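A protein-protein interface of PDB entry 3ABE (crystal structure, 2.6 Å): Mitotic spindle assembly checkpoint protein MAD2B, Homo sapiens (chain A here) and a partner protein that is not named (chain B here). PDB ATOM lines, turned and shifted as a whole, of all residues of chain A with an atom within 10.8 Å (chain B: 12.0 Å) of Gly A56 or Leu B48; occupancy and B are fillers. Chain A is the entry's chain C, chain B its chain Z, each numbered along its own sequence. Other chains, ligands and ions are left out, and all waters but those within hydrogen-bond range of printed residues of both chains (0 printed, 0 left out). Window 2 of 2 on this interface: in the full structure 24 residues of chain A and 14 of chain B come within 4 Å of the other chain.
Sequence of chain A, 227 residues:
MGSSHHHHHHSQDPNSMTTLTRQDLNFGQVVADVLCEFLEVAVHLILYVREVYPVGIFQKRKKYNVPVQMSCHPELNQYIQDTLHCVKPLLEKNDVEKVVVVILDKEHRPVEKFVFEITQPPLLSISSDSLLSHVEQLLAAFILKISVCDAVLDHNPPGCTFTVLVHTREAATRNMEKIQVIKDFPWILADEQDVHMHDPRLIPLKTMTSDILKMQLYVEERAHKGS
Of the 11 printed residues of chain B, 4 touch a printed residue of chain A.
Of the 21 printed residues of chain A, 5 touch a printed residue of chain B.
Along chain A the printed residues that touch a printed residue of chain B span positions 53 to 76.
Among the printed residues, 7 pairs touch across the chains.
O of Ile A57 is in hydrogen-bond range of N of Cys A72 (2.7 Å).
N of His A73 sits at hydrogen-bond distance from OG of Ser A71 (3.0 Å).
A ring nitrogen (ND1) of His A73 sits at hydrogen-bond distance from the backbone NH (N) of Leu A76 (3.5 Å).
The backbone carbonyl oxygen (O) of Ile B44 is in hydrogen-bond range of the side-chain hydroxyl (OG1) of Thr B47, at 2.9 Å.
Among the printed residues, merely in contact across the chains: Gly A56 with Leu B48 (3.8 Å), Ile A57 with Ile B44 (3.5 Å), Ile A57 with Leu B48 (3.5 Å), His A73 with Ile B44 (2.9 Å), His A73 with Thr B47 (3.9 Å) and Leu A76 with Pro B39 (3.7 Å).
The backbone carbonyl oxygen (O) of Pro B39 sits at hydrogen-bond distance from the side-chain hydroxyl (OH) of Tyr A53 (2.9 Å).
Gly A56 touches just one residue of chain B: Leu B48.
No residue of chain B comes within 4 Å of Pro A54.
Phe A58 touches none of the printed residues of chain B.
No residue of chain B comes within 4 Å of Cys A72.
No residue of chain A comes within 4 Å of Ala B46.
Thr B47 touches one residue of chain A.
No residue of chain A comes within 4 Å of Leu B49.
Printed residues of chain B within 4 Å of Leu A76: Pro B39 (3.7 Å).
Printed residues of chain B within 4 Å of His A73: Ile B44 (2.9 Å) and Thr B47 (3.9 Å).
Printed residues of chain A within 4 Å of Ile B44: Ile A57 and His A73.
Of the printed residues of chain B, Tyr A53 touches Pro B39 (2.9 Å).
Of the printed residues of chain A, Pro B39 touches Tyr A53 and Leu A76.
Glu A75 touches none of the printed residues of chain B.
The nearest residue of chain B that does not touch Gly A56 is Leu B49 (6.8 Å).
The nearest printed residue of chain A that does not touch Pro B39 is Glu A75 (4.1 Å).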
ATOM      1  N   LEU A  47      21.978 -20.148   1.146  1.00  0.00           N
ATOM      2  CA  LEU A  47      21.116 -19.215   1.818  1.00  0.00           C
ATOM      3  C   LEU A  47      20.981 -19.617   3.251  1.00  0.00           C
ATOM      4  O   LEU A  47      20.992 -18.778   4.128  1.00  0.00           O
ATOM      5  CB  LEU A  47      19.730 -19.233   1.165  1.00  0.00           C
ATOM      6  CG  LEU A  47      19.452 -18.461  -0.131  1.00  0.00           C
ATOM      7  CD1 LEU A  47      17.949 -18.366  -0.309  1.00  0.00           C
ATOM      8  CD2 LEU A  47      20.041 -17.054  -0.109  1.00  0.00           C
ATOM      9  N   TYR A  48      20.794 -20.917   3.466  1.00  0.00           N
ATOM     10  CA  TYR A  48      20.820 -21.564   4.789  1.00  0.00           C
ATOM     11  C   TYR A  48      22.187 -21.406   5.464  1.00  0.00           C
ATOM     12  O   TYR A  48      22.331 -20.803   6.505  1.00  0.00           O
ATOM     13  CB  TYR A  48      20.548 -23.046   4.566  1.00  0.00           C
ATOM     14  CG  TYR A  48      20.576 -23.890   5.784  1.00  0.00           C
ATOM     15  CD1 TYR A  48      19.425 -24.064   6.555  1.00  0.00           C
ATOM     16  CD2 TYR A  48      21.741 -24.553   6.173  1.00  0.00           C
ATOM     17  CE1 TYR A  48      19.444 -24.870   7.705  1.00  0.00           C
ATOM     18  CE2 TYR A  48      21.783 -25.333   7.316  1.00  0.00           C
ATOM     19  CZ  TYR A  48      20.631 -25.493   8.075  1.00  0.00           C
ATOM     20  OH  TYR A  48      20.644 -26.279   9.205  1.00  0.00           O
ATOM     21  N   VAL A  49      23.183 -22.003   4.857  1.00  0.00           N
ATOM     22  CA  VAL A  49      24.547 -21.955   5.363  1.00  0.00           C
ATOM     23  C   VAL A  49      25.086 -20.543   5.716  1.00  0.00           C
ATOM     24  O   VAL A  49      25.868 -20.423   6.622  1.00  0.00           O
ATOM     25  CB  VAL A  49      25.480 -22.647   4.362  1.00  0.00           C
ATOM     26  CG1 VAL A  49      26.816 -22.074   4.431  1.00  0.00           C
ATOM     27  CG2 VAL A  49      25.500 -24.157   4.666  1.00  0.00           C
ATOM     28  N   GLU A  51      22.960 -18.158   6.693  1.00  0.00           N
ATOM     29  CA  GLU A  51      21.785 -17.663   7.418  1.00  0.00           C
ATOM     30  C   GLU A  51      21.228 -16.424   6.751  1.00  0.00           C
ATOM     31  O   GLU A  51      21.064 -15.391   7.406  1.00  0.00           O
ATOM     32  CB  GLU A  51      22.149 -17.307   8.863  1.00  0.00           C
ATOM     33  CG  GLU A  51      22.254 -18.451   9.856  1.00  0.00           C
ATOM     34  CD  GLU A  51      23.266 -18.134  10.960  1.00  0.00           C
ATOM     35  OE1 GLU A  51      24.476 -18.328  10.728  1.00  0.00           O
ATOM     36  OE2 GLU A  51      22.867 -17.672  12.050  1.00  0.00           O
ATOM     37  N   VAL A  52      20.977 -16.475   5.450  1.00  0.00           N
ATOM     38  CA  VAL A  52      20.360 -15.313   4.815  1.00  0.00           C
ATOM     39  C   VAL A  52      18.904 -15.266   5.173  1.00  0.00           C
ATOM     40  O   VAL A  52      18.326 -14.204   5.204  1.00  0.00           O
ATOM     41  CB  VAL A  52      20.486 -15.302   3.309  1.00  0.00           C
ATOM     42  CG1 VAL A  52      19.792 -14.066   2.770  1.00  0.00           C
ATOM     43  CG2 VAL A  52      21.967 -15.329   2.903  1.00  0.00           C
ATOM     44  N   TYR A  53      18.324 -16.437   5.408  1.00  0.00           N
ATOM     45  CA  TYR A  53      16.981 -16.572   5.956  1.00  0.00           C
ATOM     46  C   TYR A  53      17.065 -17.535   7.147  1.00  0.00           C
ATOM     47  O   TYR A  53      17.985 -18.349   7.220  1.00  0.00           O
ATOM     48  CB  TYR A  53      16.012 -17.118   4.895  1.00  0.00           C
ATOM     49  CG  TYR A  53      15.832 -16.197   3.688  1.00  0.00           C
ATOM     50  CD1 TYR A  53      14.781 -15.268   3.621  1.00  0.00           C
ATOM     51  CD2 TYR A  53      16.700 -16.267   2.611  1.00  0.00           C
ATOM     52  CE1 TYR A  53      14.620 -14.430   2.510  1.00  0.00           C
ATOM     53  CE2 TYR A  53      16.557 -15.433   1.497  1.00  0.00           C
ATOM     54  CZ  TYR A  53      15.524 -14.512   1.452  1.00  0.00           C
ATOM     55  OH  TYR A  53      15.416 -13.710   0.329  1.00  0.00           O
ATOM     56  N   PRO A  54      16.158 -17.406   8.115  1.00  0.00           N
ATOM     57  CA  PRO A  54      15.939 -18.329   9.249  1.00  0.00           C
ATOM     58  C   PRO A  54      15.772 -19.833   8.932  1.00  0.00           C
ATOM     59  O   PRO A  54      15.224 -20.226   7.905  1.00  0.00           O
ATOM     60  CB  PRO A  54      14.640 -17.797   9.892  1.00  0.00           C
ATOM     61  CG  PRO A  54      14.606 -16.350   9.568  1.00  0.00           C
ATOM     62  CD  PRO A  54      15.368 -16.170   8.255  1.00  0.00           C
ATOM     63  N   VAL A  55      16.180 -20.653   9.882  1.00  0.00           N
ATOM     64  CA  VAL A  55      16.263 -22.082   9.695  1.00  0.00           C
ATOM     65  C   VAL A  55      14.906 -22.762   9.588  1.00  0.00           C
ATOM     66  O   VAL A  55      14.785 -23.850   9.038  1.00  0.00           O
ATOM     67  CB  VAL A  55      17.045 -22.682  10.871  1.00  0.00           C
ATOM     68  CG1 VAL A  55      16.811 -24.191  10.986  1.00  0.00           C
ATOM     69  CG2 VAL A  55      18.560 -22.322  10.744  1.00  0.00           C
ATOM     70  N   GLY A  56      13.879 -22.119  10.121  1.00  0.00           N
ATOM     71  CA  GLY A  56      12.570 -22.745  10.255  1.00  0.00           C
ATOM     72  C   GLY A  56      11.774 -22.842   8.967  1.00  0.00           C
ATOM     73  O   GLY A  56      10.766 -23.569   8.905  1.00  0.00           O
ATOM     74  N   ILE A  57      12.194 -22.096   7.956  1.00  0.00           N
ATOM     75  CA  ILE A  57      11.580 -22.189   6.639  1.00  0.00           C
ATOM     76  C   ILE A  57      12.238 -23.230   5.776  1.00  0.00           C
ATOM     77  O   ILE A  57      11.791 -23.435   4.663  1.00  0.00           O
ATOM     78  CB  ILE A  57      11.651 -20.878   5.805  1.00  0.00           C
ATOM     79  CG1 ILE A  57      13.090 -20.418   5.565  1.00  0.00           C
ATOM     80  CG2 ILE A  57      10.860 -19.763   6.433  1.00  0.00           C
ATOM     81  CD1 ILE A  57      13.154 -19.423   4.365  1.00  0.00           C
ATOM     82  N   PHE A  58      13.315 -23.843   6.257  1.00  0.00           N
ATOM     83  CA  PHE A  58      14.021 -24.831   5.477  1.00  0.00           C
ATOM     84  C   PHE A  58      13.627 -26.213   5.945  1.00  0.00           C
ATOM     85  O   PHE A  58      13.239 -26.416   7.091  1.00  0.00           O
ATOM     86  CB  PHE A  58      15.505 -24.683   5.631  1.00  0.00           C
ATOM     87  CG  PHE A  58      16.057 -23.464   4.979  1.00  0.00           C
ATOM     88  CD1 PHE A  58      16.401 -23.478   3.642  1.00  0.00           C
ATOM     89  CD2 PHE A  58      16.291 -22.310   5.713  1.00  0.00           C
ATOM     90  CE1 PHE A  58      16.937 -22.362   3.034  1.00  0.00           C
ATOM     91  CE2 PHE A  58      16.818 -21.190   5.120  1.00  0.00           C
ATOM     92  CZ  PHE A  58      17.151 -21.212   3.778  1.00  0.00           C
ATOM     93  N   GLN A  59      13.755 -27.167   5.035  1.00  0.00           N
ATOM     94  CA  GLN A  59      13.501 -28.551   5.317  1.00  0.00           C
ATOM     95  C   GLN A  59      14.701 -29.316   4.802  1.00  0.00           C
ATOM     96  O   GLN A  59      15.364 -28.912   3.833  1.00  0.00           O
ATOM     97  CB  GLN A  59      12.233 -28.984   4.597  1.00  0.00           C
ATOM     98  CG  GLN A  59      11.658 -30.326   5.053  1.00  0.00           C
ATOM     99  CD  GLN A  59      10.848 -31.034   3.936  1.00  0.00           C
ATOM    100  OE1 GLN A  59       9.634 -31.203   4.044  1.00  0.00           O
ATOM    101  NE2 GLN A  59      11.543 -31.419   2.845  1.00  0.00           N
ATOM    102  N   LYS A  60      14.992 -30.432   5.414  1.00  0.00           N
ATOM    103  CA  LYS A  60      16.053 -31.210   4.890  1.00  0.00           C
ATOM    104  C   LYS A  60      15.482 -32.043   3.809  1.00  0.00           C
ATOM    105  O   LYS A  60      14.479 -32.675   3.958  1.00  0.00           O
ATOM    106  CB  LYS A  60      16.683 -32.052   5.971  1.00  0.00           C
ATOM    107  N   GLN A  69      19.390 -28.485   2.470  1.00  0.00           N
ATOM    108  CA  GLN A  69      18.349 -27.678   3.038  1.00  0.00           C
ATOM    109  C   GLN A  69      17.773 -26.872   1.905  1.00  0.00           C
ATOM    110  O   GLN A  69      18.476 -26.089   1.254  1.00  0.00           O
ATOM    111  CB  GLN A  69      18.880 -26.766   4.149  1.00  0.00           C
ATOM    112  CG  GLN A  69      19.350 -27.532   5.427  1.00  0.00           C
ATOM    113  CD  GLN A  69      18.198 -28.017   6.324  1.00  0.00           C
ATOM    114  OE1 GLN A  69      17.113 -27.418   6.394  1.00  0.00           O
ATOM    115  NE2 GLN A  69      18.444 -29.102   7.023  1.00  0.00           N
ATOM    116  N   MET A  70      16.489 -27.111   1.659  1.00  0.00           N
ATOM    117  CA  MET A  70      15.719 -26.360   0.703  1.00  0.00           C
ATOM    118  C   MET A  70      14.638 -25.631   1.470  1.00  0.00           C
ATOM    119  O   MET A  70      14.169 -26.104   2.504  1.00  0.00           O
ATOM    120  CB  MET A  70      15.026 -27.255  -0.325  1.00  0.00           C
ATOM    121  CG  MET A  70      15.824 -28.362  -0.930  1.00  0.00           C
ATOM    122  SD  MET A  70      17.040 -27.834  -2.127  1.00  0.00           S
ATOM    123  CE  MET A  70      15.886 -27.454  -3.460  1.00  0.00           C
ATOM    124  N   SER A  71      14.198 -24.536   0.875  1.00  0.00           N
ATOM    125  CA  SER A  71      13.334 -23.576   1.455  1.00  0.00           C
ATOM    126  C   SER A  71      11.921 -23.987   1.107  1.00  0.00           C
ATOM    127  O   SER A  71      11.628 -24.359  -0.052  1.00  0.00           O
ATOM    128  CB  SER A  71      13.610 -22.211   0.829  1.00  0.00           C
ATOM    129  OG  SER A  71      12.422 -21.534   0.476  1.00  0.00           O
ATOM    130  N   CYS A  72      11.043 -23.881   2.095  1.00  0.00           N
ATOM    131  CA  CYS A  72       9.637 -24.076   1.879  1.00  0.00           C
ATOM    132  C   CYS A  72       8.889 -22.760   1.792  1.00  0.00           C
ATOM    133  O   CYS A  72       7.696 -22.727   2.018  1.00  0.00           O
ATOM    134  CB  CYS A  72       9.072 -24.917   2.993  1.00  0.00           C
ATOM    135  SG  CYS A  72      10.000 -26.462   3.172  1.00  0.00           S
ATOM    136  N   HIS A  73       9.563 -21.668   1.423  1.00  0.00           N
ATOM    137  CA  HIS A  73       8.815 -20.442   1.245  1.00  0.00           C
ATOM    138  C   HIS A  73       8.602 -20.220  -0.225  1.00  0.00           C
ATOM    139  O   HIS A  73       9.547 -19.921  -0.939  1.00  0.00           O
ATOM    140  CB  HIS A  73       9.512 -19.257   1.859  1.00  0.00           C
ATOM    141  CG  HIS A  73       8.674 -18.018   1.892  1.00  0.00           C
ATOM    142  ND1 HIS A  73       8.900 -16.947   1.051  1.00  0.00           N
ATOM    143  CD2 HIS A  73       7.612 -17.684   2.661  1.00  0.00           C
ATOM    144  CE1 HIS A  73       8.016 -16.000   1.315  1.00  0.00           C
ATOM    145  NE2 HIS A  73       7.220 -16.427   2.278  1.00  0.00           N
ATOM    146  N   PRO A  74       7.340 -20.324  -0.672  1.00  0.00           N
ATOM    147  CA  PRO A  74       7.026 -20.377  -2.106  1.00  0.00           C
ATOM    148  C   PRO A  74       7.429 -19.181  -2.912  1.00  0.00           C
ATOM    149  O   PRO A  74       7.799 -19.350  -4.040  1.00  0.00           O
ATOM    150  CB  PRO A  74       5.461 -20.552  -2.162  1.00  0.00           C
ATOM    151  CG  PRO A  74       5.007 -20.523  -0.782  1.00  0.00           C
ATOM    152  CD  PRO A  74       6.144 -20.436   0.186  1.00  0.00           C
ATOM    153  N   GLU A  75       7.252 -17.987  -2.381  1.00  0.00           N
ATOM    154  CA  GLU A  75       7.691 -16.802  -3.087  1.00  0.00           C
ATOM    155  C   GLU A  75       9.187 -16.891  -3.274  1.00  0.00           C
ATOM    156  O   GLU A  75       9.668 -16.621  -4.381  1.00  0.00           O
ATOM    157  CB  GLU A  75       7.371 -15.519  -2.355  1.00  0.00           C
ATOM    158  CG  GLU A  75       5.892 -15.162  -2.391  1.00  0.00           C
ATOM    159  CD  GLU A  75       5.014 -16.179  -1.646  1.00  0.00           C
ATOM    160  OE1 GLU A  75       5.596 -17.099  -1.013  1.00  0.00           O
ATOM    161  OE2 GLU A  75       3.754 -16.054  -1.686  1.00  0.00           O
ATOM    162  N   LEU A  76       9.927 -17.308  -2.240  1.00  0.00           N
ATOM    163  CA  LEU A  76      11.372 -17.379  -2.406  1.00  0.00           C
ATOM    164  C   LEU A  76      11.749 -18.432  -3.428  1.00  0.00           C
ATOM    165  O   LEU A  76      12.780 -18.324  -4.139  1.00  0.00           O
ATOM    166  CB  LEU A  76      12.083 -17.707  -1.091  1.00  0.00           C
ATOM    167  CG  LEU A  76      13.620 -17.810  -1.221  1.00  0.00           C
ATOM    168  CD1 LEU A  76      14.219 -16.551  -1.779  1.00  0.00           C
ATOM    169  CD2 LEU A  76      14.266 -18.140   0.144  1.00  0.00           C
ATOM    170  N   PRO B  39      11.948 -11.819  -1.569  1.00  0.00           N
ATOM    171  CA  PRO B  39      11.245 -11.642  -0.311  1.00  0.00           C
ATOM    172  C   PRO B  39      12.195 -11.327   0.812  1.00  0.00           C
ATOM    173  O   PRO B  39      13.209 -12.004   0.944  1.00  0.00           O
ATOM    174  CB  PRO B  39      10.628 -13.014  -0.069  1.00  0.00           C
ATOM    175  CG  PRO B  39      11.048 -13.874  -1.240  1.00  0.00           C
ATOM    176  CD  PRO B  39      11.403 -12.961  -2.307  1.00  0.00           C
ATOM    177  N   SER B  40      11.879 -10.311   1.606  1.00  0.00           N
ATOM    178  CA  SER B  40      12.713  -9.923   2.749  1.00  0.00           C
ATOM    179  C   SER B  40      12.557 -10.930   3.846  1.00  0.00           C
ATOM    180  O   SER B  40      11.643 -11.733   3.791  1.00  0.00           O
ATOM    181  CB  SER B  40      12.225  -8.612   3.313  1.00  0.00           C
ATOM    182  OG  SER B  40      10.877  -8.784   3.682  1.00  0.00           O
ATOM    183  N   ARG B  41      13.413 -10.855   4.863  1.00  0.00           N
ATOM    184  CA  ARG B  41      13.289 -11.738   6.031  1.00  0.00           C
ATOM    185  C   ARG B  41      11.952 -11.494   6.746  1.00  0.00           C
ATOM    186  O   ARG B  41      11.238 -12.443   7.040  1.00  0.00           O
ATOM    187  CB  ARG B  41      14.475 -11.576   6.998  1.00  0.00           C
ATOM    188  N   GLU B  42      11.582 -10.260   6.983  1.00  0.00           N
ATOM    189  CA  GLU B  42      10.317 -10.017   7.617  1.00  0.00           C
ATOM    190  C   GLU B  42       9.172 -10.674   6.865  1.00  0.00           C
ATOM    191  O   GLU B  42       8.458 -11.487   7.396  1.00  0.00           O
ATOM    192  CB  GLU B  42      10.089  -8.524   7.764  1.00  0.00           C
ATOM    193  N   GLU B  43       8.986 -10.319   5.617  1.00  0.00           N
ATOM    194  CA  GLU B  43       7.884 -10.887   4.840  1.00  0.00           C
ATOM    195  C   GLU B  43       7.690 -12.386   5.085  1.00  0.00           C
ATOM    196  O   GLU B  43       6.570 -12.900   5.065  1.00  0.00           O
ATOM    197  CB  GLU B  43       8.110 -10.630   3.352  1.00  0.00           C
ATOM    198  CG  GLU B  43       7.692  -9.237   2.930  1.00  0.00           C
ATOM    199  CD  GLU B  43       8.243  -8.822   1.559  1.00  0.00           C
ATOM    200  OE1 GLU B  43       8.347  -7.576   1.353  1.00  0.00           O
ATOM    201  OE2 GLU B  43       8.557  -9.712   0.706  1.00  0.00           O
ATOM    202  N   ILE B  44       8.796 -13.061   5.345  1.00  0.00           N
ATOM    203  CA  ILE B  44       8.820 -14.503   5.502  1.00  0.00           C
ATOM    204  C   ILE B  44       8.386 -14.971   6.894  1.00  0.00           C
ATOM    205  O   ILE B  44       7.853 -16.070   7.053  1.00  0.00           O
ATOM    206  CB  ILE B  44      10.238 -15.021   5.267  1.00  0.00           C
ATOM    207  CG1 ILE B  44      10.791 -14.495   3.935  1.00  0.00           C
ATOM    208  CG2 ILE B  44      10.242 -16.523   5.262  1.00  0.00           C
ATOM    209  CD1 ILE B  44      10.728 -15.469   2.811  1.00  0.00           C
ATOM    210  N   MET B  45       8.626 -14.124   7.891  1.00  0.00           N
ATOM    211  CA  MET B  45       8.406 -14.463   9.284  1.00  0.00           C
ATOM    212  C   MET B  45       6.928 -14.526   9.553  1.00  0.00           C
ATOM    213  O   MET B  45       6.482 -15.285  10.412  1.00  0.00           O
ATOM    214  CB  MET B  45       9.006 -13.392  10.202  1.00  0.00           C
ATOM    215  CG  MET B  45      10.445 -12.972   9.887  1.00  0.00           C
ATOM    216  SD  MET B  45      11.709 -13.487  11.081  1.00  0.00           S
ATOM    217  CE  MET B  45      11.346 -12.436  12.532  1.00  0.00           C
ATOM    218  N   ALA B  46       6.173 -13.702   8.829  1.00  0.00           N
ATOM    219  CA  ALA B  46       4.736 -13.571   9.042  1.00  0.00           C
ATOM    220  C   ALA B  46       4.012 -14.911   8.938  1.00  0.00           C
ATOM    221  O   ALA B  46       2.973 -15.109   9.571  1.00  0.00           O
ATOM    222  CB  ALA B  46       4.156 -12.572   8.046  1.00  0.00           C
ATOM    223  N   THR B  47       4.580 -15.827   8.153  1.00  0.00           N
ATOM    224  CA  THR B  47       3.951 -17.107   7.848  1.00  0.00           C
ATOM    225  C   THR B  47       4.402 -18.269   8.753  1.00  0.00           C
ATOM    226  O   THR B  47       3.892 -19.389   8.642  1.00  0.00           O
ATOM    227  CB  THR B  47       4.137 -17.474   6.336  1.00  0.00           C
ATOM    228  OG1 THR B  47       5.526 -17.496   5.964  1.00  0.00           O
ATOM    229  CG2 THR B  47       3.385 -16.480   5.448  1.00  0.00           C
ATOM    230  N   LEU B  48       5.298 -17.987   9.696  1.00  0.00           N
ATOM    231  CA  LEU B  48       5.905 -19.030  10.509  1.00  0.00           C
ATOM    232  C   LEU B  48       5.529 -19.010  11.966  1.00  0.00           C
ATOM    233  O   LEU B  48       5.071 -18.003  12.477  1.00  0.00           O
ATOM    234  CB  LEU B  48       7.413 -18.929  10.406  1.00  0.00           C
ATOM    235  CG  LEU B  48       8.065 -19.933   9.458  1.00  0.00           C
ATOM    236  CD1 LEU B  48       9.559 -19.806   9.641  1.00  0.00           C
ATOM    237  CD2 LEU B  48       7.563 -21.403   9.701  1.00  0.00           C
ATOM    238  N   LEU B  49       5.771 -20.153  12.613  1.00  0.00           N
ATOM    239  CA  LEU B  49       5.514 -20.367  14.041  1.00  0.00           C
ATOM    240  C   LEU B  49       6.779 -20.849  14.762  1.00  0.00           C
ATOM    241  O   LEU B  49       7.263 -21.965  14.525  1.00  0.00           O
ATOM    242  CB  LEU B  49       4.409 -21.411  14.231  1.00  0.00           C
ATOM    243  CG  LEU B  49       3.291 -21.405  13.193  1.00  0.00           C
ATOM    244  CD1 LEU B  49       2.159 -22.341  13.612  1.00  0.00           C
ATOM    245  CD2 LEU B  49       2.787 -20.001  13.003  1.00  0.00           C
